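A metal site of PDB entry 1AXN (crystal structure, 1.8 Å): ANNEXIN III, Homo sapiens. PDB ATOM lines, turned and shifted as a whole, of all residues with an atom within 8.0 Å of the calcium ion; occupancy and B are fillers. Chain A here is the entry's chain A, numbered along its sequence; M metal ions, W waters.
Four residues have an atom within 4 Å of the calcium ion: Gly 186, Arg 189, Gly 191 and Glu 231.
The nearest printed residue that does not touch the calcium ion is Trp 190 (4.1 Å).
The backbone carbonyl oxygen (O) of Glu 231 sits at hydrogen-bond distance from the side-chain hydroxyl (OG1) of Thr 192.
The calcium ion is bound by the backbone carbonyl oxygen (O) of Gly 191, the backbone carbonyl oxygen (O) of Gly 186, the backbone carbonyl oxygen (O) of Arg 189, the side-chain carboxylate (OE1) of Glu 231, the side-chain carboxylate (OE2) of Glu 231, water W2 and water W1.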
ATOM      1  N   LEU A 182      -4.415  22.445 -13.892  1.00  0.00           N
ATOM      2  CA  LEU A 182      -3.301  22.347 -14.817  1.00  0.00           C
ATOM      3  C   LEU A 182      -3.765  21.865 -16.190  1.00  0.00           C
ATOM      4  O   LEU A 182      -3.286  22.299 -17.241  1.00  0.00           O
ATOM      5  CB  LEU A 182      -2.215  21.412 -14.275  1.00  0.00           C
ATOM      6  CG  LEU A 182      -1.350  22.026 -13.162  1.00  0.00           C
ATOM      7  CD1 LEU A 182      -0.525  20.946 -12.457  1.00  0.00           C
ATOM      8  CD2 LEU A 182      -0.456  23.123 -13.699  1.00  0.00           C
ATOM      9  N   TYR A 183      -4.723  20.920 -16.134  1.00  0.00           N
ATOM     10  CA  TYR A 183      -5.266  20.349 -17.374  1.00  0.00           C
ATOM     11  C   TYR A 183      -5.961  21.423 -18.203  1.00  0.00           C
ATOM     12  O   TYR A 183      -5.748  21.602 -19.385  1.00  0.00           O
ATOM     13  CB  TYR A 183      -6.192  19.169 -17.013  1.00  0.00           C
ATOM     14  CG  TYR A 183      -6.580  18.425 -18.283  1.00  0.00           C
ATOM     15  CD1 TYR A 183      -5.616  17.779 -19.022  1.00  0.00           C
ATOM     16  CD2 TYR A 183      -7.900  18.404 -18.729  1.00  0.00           C
ATOM     17  CE1 TYR A 183      -5.947  17.108 -20.179  1.00  0.00           C
ATOM     18  CE2 TYR A 183      -8.241  17.738 -19.897  1.00  0.00           C
ATOM     19  CZ  TYR A 183      -7.253  17.089 -20.608  1.00  0.00           C
ATOM     20  OH  TYR A 183      -7.570  16.417 -21.779  1.00  0.00           O
ATOM     21  N   LYS A 184      -6.819  22.173 -17.539  1.00  0.00           N
ATOM     22  CA  LYS A 184      -7.585  23.270 -18.106  1.00  0.00           C
ATOM     23  C   LYS A 184      -6.701  24.435 -18.542  1.00  0.00           C
ATOM     24  O   LYS A 184      -7.050  25.143 -19.498  1.00  0.00           O
ATOM     25  CB  LYS A 184      -8.650  23.678 -17.075  1.00  0.00           C
ATOM     26  CG  LYS A 184      -9.370  24.973 -17.361  1.00  0.00           C
ATOM     27  CD  LYS A 184      -8.751  26.245 -16.828  1.00  0.00           C
ATOM     28  CE  LYS A 184      -9.524  26.916 -15.714  1.00  0.00           C
ATOM     29  NZ  LYS A 184      -9.162  26.382 -14.360  1.00  0.00           N
ATOM     30  N   ALA A 185      -5.571  24.667 -17.869  1.00  0.00           N
ATOM     31  CA  ALA A 185      -4.650  25.751 -18.163  1.00  0.00           C
ATOM     32  C   ALA A 185      -3.675  25.432 -19.306  1.00  0.00           C
ATOM     33  O   ALA A 185      -2.972  26.315 -19.773  1.00  0.00           O
ATOM     34  CB  ALA A 185      -3.774  26.106 -16.947  1.00  0.00           C
ATOM     35  N   GLY A 186      -3.639  24.185 -19.728  1.00  0.00           N
ATOM     36  CA  GLY A 186      -2.729  23.798 -20.754  1.00  0.00           C
ATOM     37  C   GLY A 186      -3.250  22.997 -21.910  1.00  0.00           C
ATOM     38  O   GLY A 186      -3.640  23.541 -22.937  1.00  0.00           O
ATOM     39  N   GLU A 187      -3.234  21.688 -21.777  1.00  0.00           N
ATOM     40  CA  GLU A 187      -3.658  20.736 -22.761  1.00  0.00           C
ATOM     41  C   GLU A 187      -5.063  20.955 -23.301  1.00  0.00           C
ATOM     42  O   GLU A 187      -5.295  20.823 -24.489  1.00  0.00           O
ATOM     43  CB  GLU A 187      -3.700  19.339 -22.126  1.00  0.00           C
ATOM     44  CG  GLU A 187      -2.334  18.848 -21.717  1.00  0.00           C
ATOM     45  CD  GLU A 187      -1.590  18.171 -22.847  1.00  0.00           C
ATOM     46  OE1 GLU A 187      -2.280  17.707 -23.768  1.00  0.00           O
ATOM     47  OE2 GLU A 187      -0.360  18.096 -22.850  1.00  0.00           O
ATOM     48  N   ASN A 188      -5.977  21.268 -22.375  1.00  0.00           N
ATOM     49  CA  ASN A 188      -7.360  21.486 -22.740  1.00  0.00           C
ATOM     50  C   ASN A 188      -7.669  22.825 -23.354  1.00  0.00           C
ATOM     51  O   ASN A 188      -8.863  23.121 -23.517  1.00  0.00           O
ATOM     52  CB  ASN A 188      -8.231  21.265 -21.491  1.00  0.00           C
ATOM     53  CG  ASN A 188      -9.574  20.719 -21.927  1.00  0.00           C
ATOM     54  OD1 ASN A 188     -10.600  21.131 -21.393  1.00  0.00           O
ATOM     55  ND2 ASN A 188      -9.571  19.800 -22.891  1.00  0.00           N
ATOM     56  N   ARG A 189      -6.679  23.656 -23.691  1.00  0.00           N
ATOM     57  CA  ARG A 189      -7.022  24.940 -24.275  1.00  0.00           C
ATOM     58  C   ARG A 189      -6.024  25.423 -25.311  1.00  0.00           C
ATOM     59  O   ARG A 189      -4.869  24.993 -25.278  1.00  0.00           O
ATOM     60  CB  ARG A 189      -7.111  26.008 -23.185  1.00  0.00           C
ATOM     61  CG  ARG A 189      -5.836  26.192 -22.374  1.00  0.00           C
ATOM     62  CD  ARG A 189      -5.896  27.534 -21.646  1.00  0.00           C
ATOM     63  NE  ARG A 189      -5.422  28.608 -22.496  1.00  0.00           N
ATOM     64  CZ  ARG A 189      -5.331  29.870 -22.130  1.00  0.00           C
ATOM     65  NH1 ARG A 189      -5.684  30.225 -20.900  1.00  0.00           N
ATOM     66  NH2 ARG A 189      -4.873  30.781 -22.994  1.00  0.00           N
ATOM     67  N   TRP A 190      -6.463  26.333 -26.196  1.00  0.00           N
ATOM     68  CA  TRP A 190      -5.520  26.880 -27.181  1.00  0.00           C
ATOM     69  C   TRP A 190      -4.558  27.728 -26.320  1.00  0.00           C
ATOM     70  O   TRP A 190      -5.069  28.390 -25.424  1.00  0.00           O
ATOM     71  CB  TRP A 190      -6.202  27.745 -28.211  1.00  0.00           C
ATOM     72  CG  TRP A 190      -7.118  26.939 -29.087  1.00  0.00           C
ATOM     73  CD1 TRP A 190      -7.150  25.594 -29.331  1.00  0.00           C
ATOM     74  CD2 TRP A 190      -8.166  27.529 -29.889  1.00  0.00           C
ATOM     75  NE1 TRP A 190      -8.171  25.318 -30.239  1.00  0.00           N
ATOM     76  CE2 TRP A 190      -8.801  26.481 -30.572  1.00  0.00           C
ATOM     77  CE3 TRP A 190      -8.587  28.852 -30.056  1.00  0.00           C
ATOM     78  CZ2 TRP A 190      -9.876  26.696 -31.435  1.00  0.00           C
ATOM     79  CZ3 TRP A 190      -9.655  29.066 -30.925  1.00  0.00           C
ATOM     80  CH2 TRP A 190     -10.272  27.989 -31.584  1.00  0.00           C
ATOM     81  N   GLY A 191      -3.281  27.662 -26.572  1.00  0.00           N
ATOM     82  CA  GLY A 191      -2.332  28.427 -25.776  1.00  0.00           C
ATOM     83  C   GLY A 191      -2.214  27.800 -24.381  1.00  0.00           C
ATOM     84  O   GLY A 191      -2.561  26.647 -24.160  1.00  0.00           O
ATOM     85  N   THR A 192      -1.728  28.614 -23.460  1.00  0.00           N
ATOM     86  CA  THR A 192      -1.507  28.157 -22.093  1.00  0.00           C
ATOM     87  C   THR A 192      -1.642  29.249 -21.041  1.00  0.00           C
ATOM     88  O   THR A 192      -1.297  30.373 -21.366  1.00  0.00           O
ATOM     89  CB  THR A 192      -0.006  27.747 -21.963  1.00  0.00           C
ATOM     90  OG1 THR A 192       0.387  26.873 -23.025  1.00  0.00           O
ATOM     91  CG2 THR A 192       0.330  27.076 -20.636  1.00  0.00           C
ATOM     92  N   ASP A 193      -2.115  28.905 -19.859  1.00  0.00           N
ATOM     93  CA  ASP A 193      -2.202  29.869 -18.768  1.00  0.00           C
ATOM     94  C   ASP A 193      -0.885  29.552 -18.014  1.00  0.00           C
ATOM     95  O   ASP A 193      -0.940  28.683 -17.144  1.00  0.00           O
ATOM     96  CB  ASP A 193      -3.377  29.759 -17.826  1.00  0.00           C
ATOM     97  CG  ASP A 193      -3.424  30.856 -16.752  1.00  0.00           C
ATOM     98  OD1 ASP A 193      -2.441  31.618 -16.653  1.00  0.00           O
ATOM     99  OD2 ASP A 193      -4.427  30.951 -16.049  1.00  0.00           O
ATOM    100  N   PHE A 197       0.629  27.445 -14.209  1.00  0.00           N
ATOM    101  CA  PHE A 197       1.657  26.404 -14.108  1.00  0.00           C
ATOM    102  C   PHE A 197       2.657  26.820 -13.017  1.00  0.00           C
ATOM    103  O   PHE A 197       3.025  26.015 -12.178  1.00  0.00           O
ATOM    104  CB  PHE A 197       2.394  26.213 -15.427  1.00  0.00           C
ATOM    105  CG  PHE A 197       1.733  25.158 -16.273  1.00  0.00           C
ATOM    106  CD1 PHE A 197       0.681  25.491 -17.124  1.00  0.00           C
ATOM    107  CD2 PHE A 197       2.176  23.849 -16.188  1.00  0.00           C
ATOM    108  CE1 PHE A 197       0.088  24.488 -17.884  1.00  0.00           C
ATOM    109  CE2 PHE A 197       1.578  22.863 -16.958  1.00  0.00           C
ATOM    110  CZ  PHE A 197       0.535  23.192 -17.798  1.00  0.00           C
ATOM    111  N   SER A 227       2.937  17.256 -20.970  1.00  0.00           N
ATOM    112  CA  SER A 227       2.163  18.499 -21.113  1.00  0.00           C
ATOM    113  C   SER A 227       3.085  19.707 -21.151  1.00  0.00           C
ATOM    114  O   SER A 227       3.003  20.597 -21.983  1.00  0.00           O
ATOM    115  CB  SER A 227       1.110  18.614 -20.002  1.00  0.00           C
ATOM    116  OG  SER A 227       0.192  17.540 -20.141  1.00  0.00           O
ATOM    117  N   GLY A 230       4.878  19.947 -24.365  1.00  0.00           N
ATOM    118  CA  GLY A 230       4.019  20.395 -25.466  1.00  0.00           C
ATOM    119  C   GLY A 230       3.528  21.827 -25.408  1.00  0.00           C
ATOM    120  O   GLY A 230       3.359  22.543 -26.420  1.00  0.00           O
ATOM    121  N   GLU A 231       3.261  22.328 -24.221  1.00  0.00           N
ATOM    122  CA  GLU A 231       2.737  23.667 -24.022  1.00  0.00           C
ATOM    123  C   GLU A 231       3.727  24.800 -23.856  1.00  0.00           C
ATOM    124  O   GLU A 231       3.464  25.946 -24.230  1.00  0.00           O
ATOM    125  CB  GLU A 231       1.904  23.593 -22.734  1.00  0.00           C
ATOM    126  CG  GLU A 231       0.693  22.668 -22.752  1.00  0.00           C
ATOM    127  CD  GLU A 231      -0.407  23.252 -23.627  1.00  0.00           C
ATOM    128  OE1 GLU A 231      -0.660  24.469 -23.503  1.00  0.00           O
ATOM    129  OE2 GLU A 231      -1.040  22.520 -24.422  1.00  0.00           O
ATOM    130  N   LEU A 232       4.895  24.493 -23.270  1.00  0.00           N
ATOM    131  CA  LEU A 232       5.899  25.516 -23.029  1.00  0.00           C
ATOM    132  C   LEU A 232       7.165  25.395 -23.842  1.00  0.00           C
ATOM    133  O   LEU A 232       7.438  24.405 -24.512  1.00  0.00           O
ATOM    134  CB  LEU A 232       6.179  25.480 -21.527  1.00  0.00           C
ATOM    135  CG  LEU A 232       4.971  25.378 -20.592  1.00  0.00           C
ATOM    136  CD1 LEU A 232       5.460  25.186 -19.168  1.00  0.00           C
ATOM    137  CD2 LEU A 232       4.046  26.573 -20.658  1.00  0.00           C
HETATM  138 CA    CA M   1      -2.621  24.457 -24.813  1.00  0.00          CA
HETATM  139  O   HOH W   1      -0.922  25.128 -26.742  1.00  0.00           O
HETATM  140  O   HOH W   2      -3.404  22.595 -26.475  1.00  0.00           O
